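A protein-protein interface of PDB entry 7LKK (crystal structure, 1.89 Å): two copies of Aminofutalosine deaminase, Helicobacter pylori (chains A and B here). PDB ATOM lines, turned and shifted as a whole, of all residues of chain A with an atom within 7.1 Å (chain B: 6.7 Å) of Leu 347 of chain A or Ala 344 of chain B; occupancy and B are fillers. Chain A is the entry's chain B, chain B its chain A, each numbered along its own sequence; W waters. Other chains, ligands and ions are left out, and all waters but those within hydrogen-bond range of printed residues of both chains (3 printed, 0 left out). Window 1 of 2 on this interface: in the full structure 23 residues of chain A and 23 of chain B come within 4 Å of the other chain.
Among the printed residues, merely in contact across the chains: Leu 356 of chain A with Arg 304 of chain B (3.5 Å), Leu 347 of chain A with Leu 347 of chain B (3.5 Å), Leu 353 of chain A with Arg 304 of chain B (3.6 Å), Leu 347 of chain A with Arg 304 of chain B (3.8 Å), Leu 347 of chain A with Ala 344 of chain B (3.8 Å), Ala 344 of chain A with Leu 347 of chain B (3.8 Å), Leu 353 of chain A with Leu 305 of chain B (3.9 Å) and Phe 301 of chain A with Leu 347 of chain B (3.9 Å).
Water W2 bridges O of Leu 347 of chain B and OG of Ser 348 of chain A.
Water W1 bridges OG of Ser 348 of chain B (2.9 Å) and O of Leu 347 of chain A (3.0 Å).
Water W3 bridges N of Leu 353 of chain A (3.1 Å) and NH1 of Arg 304 of chain B (3.3 Å).
Of the 13 printed residues of chain A, 7 touch a printed residue of chain B.
Hydrophobic or aromatic side chains of chain A within 4 Å of the printed part of chain B: Phe 301, Ala 344, Leu 347, Leu 353 and Leu 356.
Hydrophobic or aromatic side chains of chain B that line the printed part of chain A: Leu 305, Ala 344 and Leu 347.
Among the printed residues, no Asp or Glu carboxylate lies within 4 Å of a Lys or Arg side-chain nitrogen of the other chain.
O of Ala 344 of chain B is in hydrogen-bond range of OG of Ser 348 of chain B, 2.7 Å away.
The side-chain carboxylate (OE2) of Glu 341 of chain A is in hydrogen-bond range of the backbone NH (N) of Phe 301 of chain A (3.0 Å).
The backbone carbonyl oxygen (O) of Ala 344 of chain A lies within hydrogen-bond range of the side-chain hydroxyl (OG) of Ser 348 of chain A (2.7 Å).
Printed residues of chain B within 4 Å of Phe 301 of chain A: Leu 347.
Of the printed residues of chain B, Leu 347 of chain A touches Arg 304, Ala 344 and Leu 347.
Of the printed residues of chain B, His 349 of chain A touches Arg 304 (3.0 Å).
Ala 344 of chain B touches one residue of chain A.
The nearest printed residue of chain A that does not touch Leu 305 of chain B is Leu 347 of chain A (6.5 Å).
Phe 301 of chain A touches Leu 347 of chain B, but with the chains exchanged Leu 347 of chain A does not touch Phe 301 of chain B (4.1 Å).
Ala 344 of chain A touches Leu 347 of chain B, and with the chains exchanged Leu 347 of chain A touches Ala 344 of chain B.
Leu 347 of chain A touches its own counterpart, Leu 347 of chain B.
10 positions are printed for both chains.
The backbone carbonyl oxygen of Leu 346 of chain A lies within hydrogen-bond range of the guanidinium group of Arg 304 of chain B, at 2.9 Å.
O of His 349 of chain A lies within hydrogen-bond range of NH2 of Arg 304 of chain B, 3.0 Å away.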
ATOM      1  N   PHE A 301     -11.779  14.727  29.838  1.00  0.00           N
ATOM      2  CA  PHE A 301     -12.876  14.020  29.183  1.00  0.00           C
ATOM      3  C   PHE A 301     -13.863  14.995  28.554  1.00  0.00           C
ATOM      4  O   PHE A 301     -14.347  14.764  27.440  1.00  0.00           O
ATOM      5  CB  PHE A 301     -13.585  13.097  30.175  1.00  0.00           C
ATOM      6  CG  PHE A 301     -14.181  11.870  29.541  1.00  0.00           C
ATOM      7  CD1 PHE A 301     -15.445  11.911  28.973  1.00  0.00           C
ATOM      8  CD2 PHE A 301     -13.478  10.679  29.508  1.00  0.00           C
ATOM      9  CE1 PHE A 301     -15.998  10.787  28.390  1.00  0.00           C
ATOM     10  CE2 PHE A 301     -14.023   9.548  28.923  1.00  0.00           C
ATOM     11  CZ  PHE A 301     -15.284   9.602  28.362  1.00  0.00           C
ATOM     12  N   GLU A 341     -11.148  10.394  35.902  1.00  0.00           N
ATOM     13  CA  GLU A 341     -10.672  11.568  35.179  1.00  0.00           C
ATOM     14  C   GLU A 341      -9.151  11.584  35.092  1.00  0.00           C
ATOM     15  O   GLU A 341      -8.583  12.004  34.077  1.00  0.00           O
ATOM     16  CB  GLU A 341     -11.183  12.841  35.854  1.00  0.00           C
ATOM     17  CG  GLU A 341     -11.158  14.068  34.963  1.00  0.00           C
ATOM     18  CD  GLU A 341     -12.170  13.987  33.837  1.00  0.00           C
ATOM     19  OE1 GLU A 341     -13.188  13.278  33.996  1.00  0.00           O
ATOM     20  OE2 GLU A 341     -11.951  14.631  32.791  1.00  0.00           O
ATOM     21  N   LEU A 342      -8.472  11.149  36.155  1.00  0.00           N
ATOM     22  CA  LEU A 342      -7.013  11.139  36.142  1.00  0.00           C
ATOM     23  C   LEU A 342      -6.475  10.118  35.143  1.00  0.00           C
ATOM     24  O   LEU A 342      -5.447  10.356  34.501  1.00  0.00           O
ATOM     25  CB  LEU A 342      -6.475  10.873  37.548  1.00  0.00           C
ATOM     26  CG  LEU A 342      -6.751  12.003  38.549  1.00  0.00           C
ATOM     27  CD1 LEU A 342      -6.304  11.624  39.951  1.00  0.00           C
ATOM     28  CD2 LEU A 342      -6.091  13.300  38.097  1.00  0.00           C
ATOM     29  N   ARG A 343      -7.148   8.971  35.008  1.00  0.00           N
ATOM     30  CA  ARG A 343      -6.757   7.995  33.993  1.00  0.00           C
ATOM     31  C   ARG A 343      -7.038   8.507  32.584  1.00  0.00           C
ATOM     32  O   ARG A 343      -6.253   8.263  31.660  1.00  0.00           O
ATOM     33  CB  ARG A 343      -7.471   6.667  34.237  1.00  0.00           C
ATOM     34  CG  ARG A 343      -6.892   5.852  35.384  1.00  0.00           C
ATOM     35  CD  ARG A 343      -7.572   4.496  35.501  1.00  0.00           C
ATOM     36  NE  ARG A 343      -8.885   4.596  36.133  1.00  0.00           N
ATOM     37  CZ  ARG A 343      -9.085   4.604  37.447  1.00  0.00           C
ATOM     38  NH1 ARG A 343      -8.054   4.519  38.277  1.00  0.00           N
ATOM     39  NH2 ARG A 343     -10.316   4.702  37.933  1.00  0.00           N
ATOM     40  N   ALA A 344      -8.163   9.200  32.389  1.00  0.00           N
ATOM     41  CA  ALA A 344      -8.409   9.840  31.100  1.00  0.00           C
ATOM     42  C   ALA A 344      -7.342  10.887  30.809  1.00  0.00           C
ATOM     43  O   ALA A 344      -6.903  11.040  29.662  1.00  0.00           O
ATOM     44  CB  ALA A 344      -9.802  10.466  31.073  1.00  0.00           C
ATOM     45  N   PHE A 345      -6.917  11.617  31.844  1.00  0.00           N
ATOM     46  CA  PHE A 345      -5.843  12.597  31.703  1.00  0.00           C
ATOM     47  C   PHE A 345      -4.557  11.938  31.223  1.00  0.00           C
ATOM     48  O   PHE A 345      -3.874  12.460  30.334  1.00  0.00           O
ATOM     49  CB  PHE A 345      -5.630  13.304  33.043  1.00  0.00           C
ATOM     50  CG  PHE A 345      -4.583  14.382  33.019  1.00  0.00           C
ATOM     51  CD1 PHE A 345      -4.846  15.612  32.439  1.00  0.00           C
ATOM     52  CD2 PHE A 345      -3.349  14.178  33.616  1.00  0.00           C
ATOM     53  CE1 PHE A 345      -3.886  16.610  32.431  1.00  0.00           C
ATOM     54  CE2 PHE A 345      -2.386  15.171  33.614  1.00  0.00           C
ATOM     55  CZ  PHE A 345      -2.655  16.387  33.020  1.00  0.00           C
ATOM     56  N   LEU A 346      -4.215  10.781  31.795  1.00  0.00           N
ATOM     57  CA  LEU A 346      -3.023  10.063  31.357  1.00  0.00           C
ATOM     58  C   LEU A 346      -3.127   9.663  29.890  1.00  0.00           C
ATOM     59  O   LEU A 346      -2.127   9.665  29.163  1.00  0.00           O
ATOM     60  CB  LEU A 346      -2.804   8.831  32.237  1.00  0.00           C
ATOM     61  CG  LEU A 346      -2.542   9.091  33.722  1.00  0.00           C
ATOM     62  CD1 LEU A 346      -2.403   7.773  34.477  1.00  0.00           C
ATOM     63  CD2 LEU A 346      -1.302   9.956  33.914  1.00  0.00           C
ATOM     64  N   LEU A 347      -4.335   9.318  29.435  1.00  0.00           N
ATOM     65  CA  LEU A 347      -4.533   8.914  28.050  1.00  0.00           C
ATOM     66  C   LEU A 347      -4.581  10.092  27.084  1.00  0.00           C
ATOM     67  O   LEU A 347      -4.366   9.896  25.883  1.00  0.00           O
ATOM     68  CB  LEU A 347      -5.823   8.101  27.920  1.00  0.00           C
ATOM     69  CG  LEU A 347      -5.844   6.751  28.636  1.00  0.00           C
ATOM     70  CD1 LEU A 347      -7.233   6.139  28.575  1.00  0.00           C
ATOM     71  CD2 LEU A 347      -4.808   5.809  28.038  1.00  0.00           C
ATOM     72  N   SER A 348      -4.839  11.303  27.576  1.00  0.00           N
ATOM     73  CA  SER A 348      -5.093  12.454  26.720  1.00  0.00           C
ATOM     74  C   SER A 348      -3.841  13.263  26.402  1.00  0.00           C
ATOM     75  O   SER A 348      -3.933  14.239  25.651  1.00  0.00           O
ATOM     76  CB  SER A 348      -6.139  13.371  27.368  1.00  0.00           C
ATOM     77  OG  SER A 348      -7.361  12.684  27.579  1.00  0.00           O
ATOM     78  N   HIS A 349      -2.686  12.899  26.954  1.00  0.00           N
ATOM     79  CA  HIS A 349      -1.456  13.643  26.722  1.00  0.00           C
ATOM     80  C   HIS A 349      -0.309  12.669  26.498  1.00  0.00           C
ATOM     81  O   HIS A 349      -0.226  11.638  27.169  1.00  0.00           O
ATOM     82  CB  HIS A 349      -1.149  14.578  27.896  1.00  0.00           C
ATOM     83  CG  HIS A 349      -2.293  15.471  28.261  1.00  0.00           C
ATOM     84  ND1 HIS A 349      -2.495  16.700  27.672  1.00  0.00           N
ATOM     85  CD2 HIS A 349      -3.308  15.304  29.142  1.00  0.00           C
ATOM     86  CE1 HIS A 349      -3.578  17.257  28.183  1.00  0.00           C
ATOM     87  NE2 HIS A 349      -4.092  16.430  29.075  1.00  0.00           N
ATOM     88  N   ASN A 350       0.571  12.998  25.551  1.00  0.00           N
ATOM     89  CA  ASN A 350       1.637  12.095  25.134  1.00  0.00           C
ATOM     90  C   ASN A 350       2.947  12.331  25.879  1.00  0.00           C
ATOM     91  O   ASN A 350       3.979  11.779  25.482  1.00  0.00           O
ATOM     92  CB  ASN A 350       1.867  12.210  23.624  1.00  0.00           C
ATOM     93  CG  ASN A 350       2.532  13.517  23.227  1.00  0.00           C
ATOM     94  OD1 ASN A 350       2.449  14.518  23.941  1.00  0.00           O
ATOM     95  ND2 ASN A 350       3.198  13.509  22.078  1.00  0.00           N
ATOM     96  N   LEU A 353       4.915   8.958  30.642  1.00  0.00           N
ATOM     97  CA  LEU A 353       3.836   8.613  31.564  1.00  0.00           C
ATOM     98  C   LEU A 353       4.237   8.827  33.020  1.00  0.00           C
ATOM     99  O   LEU A 353       3.435   9.316  33.823  1.00  0.00           O
ATOM    100  CB  LEU A 353       3.403   7.167  31.325  1.00  0.00           C
ATOM    101  CG  LEU A 353       2.146   6.672  32.038  1.00  0.00           C
ATOM    102  CD1 LEU A 353       0.999   7.648  31.838  1.00  0.00           C
ATOM    103  CD2 LEU A 353       1.763   5.288  31.533  1.00  0.00           C
ATOM    104  N   LEU A 356       4.041  12.398  33.611  1.00  0.00           N
ATOM    105  CA  LEU A 356       2.651  12.839  33.580  1.00  0.00           C
ATOM    106  C   LEU A 356       1.885  12.388  34.817  1.00  0.00           C
ATOM    107  O   LEU A 356       0.938  13.063  35.237  1.00  0.00           O
ATOM    108  CB  LEU A 356       1.970  12.322  32.310  1.00  0.00           C
ATOM    109  CG  LEU A 356       0.584  12.882  31.985  1.00  0.00           C
ATOM    110  CD1 LEU A 356       0.644  14.389  31.838  1.00  0.00           C
ATOM    111  CD2 LEU A 356       0.025  12.242  30.719  1.00  0.00           C
ATOM    112  N   PRO B 300      -4.835   0.319  22.448  1.00  0.00           N
ATOM    113  CA  PRO B 300      -4.527   1.682  22.922  1.00  0.00           C
ATOM    114  C   PRO B 300      -3.991   1.756  24.345  1.00  0.00           C
ATOM    115  O   PRO B 300      -3.046   2.513  24.599  1.00  0.00           O
ATOM    116  CB  PRO B 300      -5.871   2.421  22.785  1.00  0.00           C
ATOM    117  CG  PRO B 300      -6.907   1.365  22.600  1.00  0.00           C
ATOM    118  CD  PRO B 300      -6.221   0.193  21.963  1.00  0.00           C
ATOM    119  N   PHE B 301      -4.575   1.017  25.292  1.00  0.00           N
ATOM    120  CA  PHE B 301      -4.124   1.144  26.676  1.00  0.00           C
ATOM    121  C   PHE B 301      -2.741   0.532  26.865  1.00  0.00           C
ATOM    122  O   PHE B 301      -1.887   1.113  27.544  1.00  0.00           O
ATOM    123  CB  PHE B 301      -5.133   0.502  27.630  1.00  0.00           C
ATOM    124  CG  PHE B 301      -5.177   1.149  28.987  1.00  0.00           C
ATOM    125  CD1 PHE B 301      -4.296   0.761  29.984  1.00  0.00           C
ATOM    126  CD2 PHE B 301      -6.093   2.151  29.263  1.00  0.00           C
ATOM    127  CE1 PHE B 301      -4.331   1.356  31.232  1.00  0.00           C
ATOM    128  CE2 PHE B 301      -6.133   2.752  30.511  1.00  0.00           C
ATOM    129  CZ  PHE B 301      -5.251   2.355  31.496  1.00  0.00           C
ATOM    130  N   ARG B 304      -0.136   2.878  25.546  1.00  0.00           N
ATOM    131  CA  ARG B 304       0.117   4.003  26.443  1.00  0.00           C
ATOM    132  C   ARG B 304       0.975   3.587  27.630  1.00  0.00           C
ATOM    133  O   ARG B 304       1.820   4.362  28.094  1.00  0.00           O
ATOM    134  CB  ARG B 304      -1.201   4.600  26.931  1.00  0.00           C
ATOM    135  CG  ARG B 304      -1.042   5.880  27.745  1.00  0.00           C
ATOM    136  CD  ARG B 304      -0.421   6.985  26.908  1.00  0.00           C
ATOM    137  NE  ARG B 304      -0.116   8.178  27.693  1.00  0.00           N
ATOM    138  CZ  ARG B 304       1.109   8.541  28.057  1.00  0.00           C
ATOM    139  NH1 ARG B 304       2.153   7.799  27.712  1.00  0.00           N
ATOM    140  NH2 ARG B 304       1.292   9.647  28.766  1.00  0.00           N
ATOM    141  N   LEU B 305       0.767   2.374  28.144  1.00  0.00           N
ATOM    142  CA  LEU B 305       1.496   1.937  29.329  1.00  0.00           C
ATOM    143  C   LEU B 305       2.931   1.540  29.012  1.00  0.00           C
ATOM    144  O   LEU B 305       3.800   1.633  29.887  1.00  0.00           O
ATOM    145  CB  LEU B 305       0.776   0.763  29.992  1.00  0.00           C
ATOM    146  CG  LEU B 305      -0.604   1.020  30.595  1.00  0.00           C
ATOM    147  CD1 LEU B 305      -1.100  -0.233  31.304  1.00  0.00           C
ATOM    148  CD2 LEU B 305      -0.573   2.205  31.548  1.00  0.00           C
ATOM    149  N   LEU B 339     -15.279  -2.744  25.960  1.00  0.00           N
ATOM    150  CA  LEU B 339     -15.901  -1.423  25.997  1.00  0.00           C
ATOM    151  C   LEU B 339     -14.990  -0.402  26.669  1.00  0.00           C
ATOM    152  O   LEU B 339     -14.902   0.748  26.220  1.00  0.00           O
ATOM    153  CB  LEU B 339     -17.248  -1.504  26.714  1.00  0.00           C
ATOM    154  CG  LEU B 339     -18.332  -2.290  25.970  1.00  0.00           C
ATOM    155  CD1 LEU B 339     -19.488  -2.635  26.894  1.00  0.00           C
ATOM    156  CD2 LEU B 339     -18.824  -1.511  24.764  1.00  0.00           C
ATOM    157  N   ASP B 340     -14.304  -0.803  27.742  1.00  0.00           N
ATOM    158  CA  ASP B 340     -13.300   0.069  28.346  1.00  0.00           C
ATOM    159  C   ASP B 340     -12.184   0.380  27.358  1.00  0.00           C
ATOM    160  O   ASP B 340     -11.723   1.524  27.268  1.00  0.00           O
ATOM    161  CB  ASP B 340     -12.725  -0.578  29.608  1.00  0.00           C
ATOM    162  CG  ASP B 340     -13.704  -0.583  30.767  1.00  0.00           C
ATOM    163  OD1 ASP B 340     -14.780   0.034  30.648  1.00  0.00           O
ATOM    164  OD2 ASP B 340     -13.393  -1.209  31.802  1.00  0.00           O
ATOM    165  N   GLU B 341     -11.743  -0.631  26.602  1.00  0.00           N
ATOM    166  CA  GLU B 341     -10.684  -0.422  25.619  1.00  0.00           C
ATOM    167  C   GLU B 341     -11.129   0.534  24.523  1.00  0.00           C
ATOM    168  O   GLU B 341     -10.335   1.354  24.043  1.00  0.00           O
ATOM    169  CB  GLU B 341     -10.260  -1.762  25.014  1.00  0.00           C
ATOM    170  CG  GLU B 341      -8.911  -1.731  24.317  1.00  0.00           C
ATOM    171  CD  GLU B 341      -7.763  -1.535  25.285  1.00  0.00           C
ATOM    172  OE1 GLU B 341      -7.906  -1.919  26.466  1.00  0.00           O
ATOM    173  OE2 GLU B 341      -6.717  -0.994  24.869  1.00  0.00           O
ATOM    174  N   LEU B 342     -12.394   0.442  24.108  1.00  0.00           N
ATOM    175  CA  LEU B 342     -12.894   1.326  23.061  1.00  0.00           C
ATOM    176  C   LEU B 342     -12.960   2.771  23.538  1.00  0.00           C
ATOM    177  O   LEU B 342     -12.665   3.695  22.773  1.00  0.00           O
ATOM    178  CB  LEU B 342     -14.265   0.847  22.583  1.00  0.00           C
ATOM    179  CG  LEU B 342     -14.240  -0.511  21.874  1.00  0.00           C
ATOM    180  CD1 LEU B 342     -15.650  -0.979  21.527  1.00  0.00           C
ATOM    181  CD2 LEU B 342     -13.360  -0.451  20.632  1.00  0.00           C
ATOM    182  N   ARG B 343     -13.334   2.987  24.801  1.00  0.00           N
ATOM    183  CA  ARG B 343     -13.321   4.343  25.343  1.00  0.00           C
ATOM    184  C   ARG B 343     -11.898   4.875  25.462  1.00  0.00           C
ATOM    185  O   ARG B 343     -11.650   6.059  25.205  1.00  0.00           O
ATOM    186  CB  ARG B 343     -14.029   4.379  26.697  1.00  0.00           C
ATOM    187  CG  ARG B 343     -15.548   4.342  26.590  1.00  0.00           C
ATOM    188  CD  ARG B 343     -16.207   4.464  27.949  1.00  0.00           C
ATOM    189  NE  ARG B 343     -16.143   3.218  28.708  1.00  0.00           N
ATOM    190  CZ  ARG B 343     -17.038   2.239  28.617  1.00  0.00           C
ATOM    191  NH1 ARG B 343     -18.074   2.354  27.794  1.00  0.00           N
ATOM    192  NH2 ARG B 343     -16.895   1.142  29.348  1.00  0.00           N
ATOM    193  N   ALA B 344     -10.947   4.019  25.849  1.00  0.00           N
ATOM    194  CA  ALA B 344      -9.548   4.432  25.830  1.00  0.00           C
ATOM    195  C   ALA B 344      -9.114   4.783  24.415  1.00  0.00           C
ATOM    196  O   ALA B 344      -8.369   5.747  24.203  1.00  0.00           O
ATOM    197  CB  ALA B 344      -8.659   3.328  26.408  1.00  0.00           C
ATOM    198  N   PHE B 345      -9.592   4.014  23.434  1.00  0.00           N
ATOM    199  CA  PHE B 345      -9.305   4.287  22.029  1.00  0.00           C
ATOM    200  C   PHE B 345      -9.800   5.673  21.627  1.00  0.00           C
ATOM    201  O   PHE B 345      -9.094   6.418  20.937  1.00  0.00           O
ATOM    202  CB  PHE B 345      -9.953   3.193  21.173  1.00  0.00           C
ATOM    203  CG  PHE B 345      -9.687   3.311  19.699  1.00  0.00           C
ATOM    204  CD1 PHE B 345      -8.470   2.922  19.163  1.00  0.00           C
ATOM    205  CD2 PHE B 345     -10.676   3.769  18.840  1.00  0.00           C
ATOM    206  CE1 PHE B 345      -8.234   3.013  17.799  1.00  0.00           C
ATOM    207  CE2 PHE B 345     -10.447   3.863  17.481  1.00  0.00           C
ATOM    208  CZ  PHE B 345      -9.224   3.484  16.960  1.00  0.00           C
ATOM    209  N   LEU B 346     -11.009   6.039  22.061  1.00  0.00           N
ATOM    210  CA  LEU B 346     -11.535   7.366  21.754  1.00  0.00           C
ATOM    211  C   LEU B 346     -10.662   8.460  22.357  1.00  0.00           C
ATOM    212  O   LEU B 346     -10.486   9.526  21.756  1.00  0.00           O
ATOM    213  CB  LEU B 346     -12.974   7.488  22.252  1.00  0.00           C
ATOM    214  CG  LEU B 346     -14.000   6.537  21.635  1.00  0.00           C
ATOM    215  CD1 LEU B 346     -15.379   6.770  22.244  1.00  0.00           C
ATOM    216  CD2 LEU B 346     -14.045   6.685  20.116  1.00  0.00           C
ATOM    217  N   LEU B 347     -10.102   8.211  23.543  1.00  0.00           N
ATOM    218  CA  LEU B 347      -9.268   9.201  24.209  1.00  0.00           C
ATOM    219  C   LEU B 347      -7.863   9.283  23.626  1.00  0.00           C
ATOM    220  O   LEU B 347      -7.187  10.299  23.818  1.00  0.00           O
ATOM    221  CB  LEU B 347      -9.176   8.889  25.704  1.00  0.00           C
ATOM    222  CG  LEU B 347     -10.478   8.985  26.500  1.00  0.00           C
ATOM    223  CD1 LEU B 347     -10.296   8.395  27.886  1.00  0.00           C
ATOM    224  CD2 LEU B 347     -10.945  10.431  26.584  1.00  0.00           C
ATOM    225  N   SER B 348      -7.419   8.254  22.907  1.00  0.00           N
ATOM    226  CA  SER B 348      -6.035   8.143  22.465  1.00  0.00           C
ATOM    227  C   SER B 348      -5.786   8.724  21.079  1.00  0.00           C
ATOM    228  O   SER B 348      -4.635   8.739  20.633  1.00  0.00           O
ATOM    229  CB  SER B 348      -5.602   6.671  22.478  1.00  0.00           C
ATOM    230  OG  SER B 348      -5.744   6.112  23.773  1.00  0.00           O
ATOM    231  N   HIS B 349      -6.819   9.203  20.388  1.00  0.00           N
ATOM    232  CA  HIS B 349      -6.659   9.722  19.037  1.00  0.00           C
ATOM    233  C   HIS B 349      -7.469  10.998  18.873  1.00  0.00           C
ATOM    234  O   HIS B 349      -8.595  11.094  19.366  1.00  0.00           O
ATOM    235  CB  HIS B 349      -7.083   8.680  17.998  1.00  0.00           C
ATOM    236  CG  HIS B 349      -6.408   7.355  18.169  1.00  0.00           C
ATOM    237  ND1 HIS B 349      -5.212   7.045  17.560  1.00  0.00           N
ATOM    238  CD2 HIS B 349      -6.757   6.263  18.890  1.00  0.00           C
ATOM    239  CE1 HIS B 349      -4.857   5.817  17.891  1.00  0.00           C
ATOM    240  NE2 HIS B 349      -5.777   5.320  18.699  1.00  0.00           N
HETATM  241  O   HOH W   1      -3.322   7.268  24.833  1.00  0.00           O
HETATM  242  O   HOH W   2      -8.327  12.387  24.631  1.00  0.00           O
HETATM  243  O   HOH W   3       5.342   7.111  28.203  1.00  0.00           O
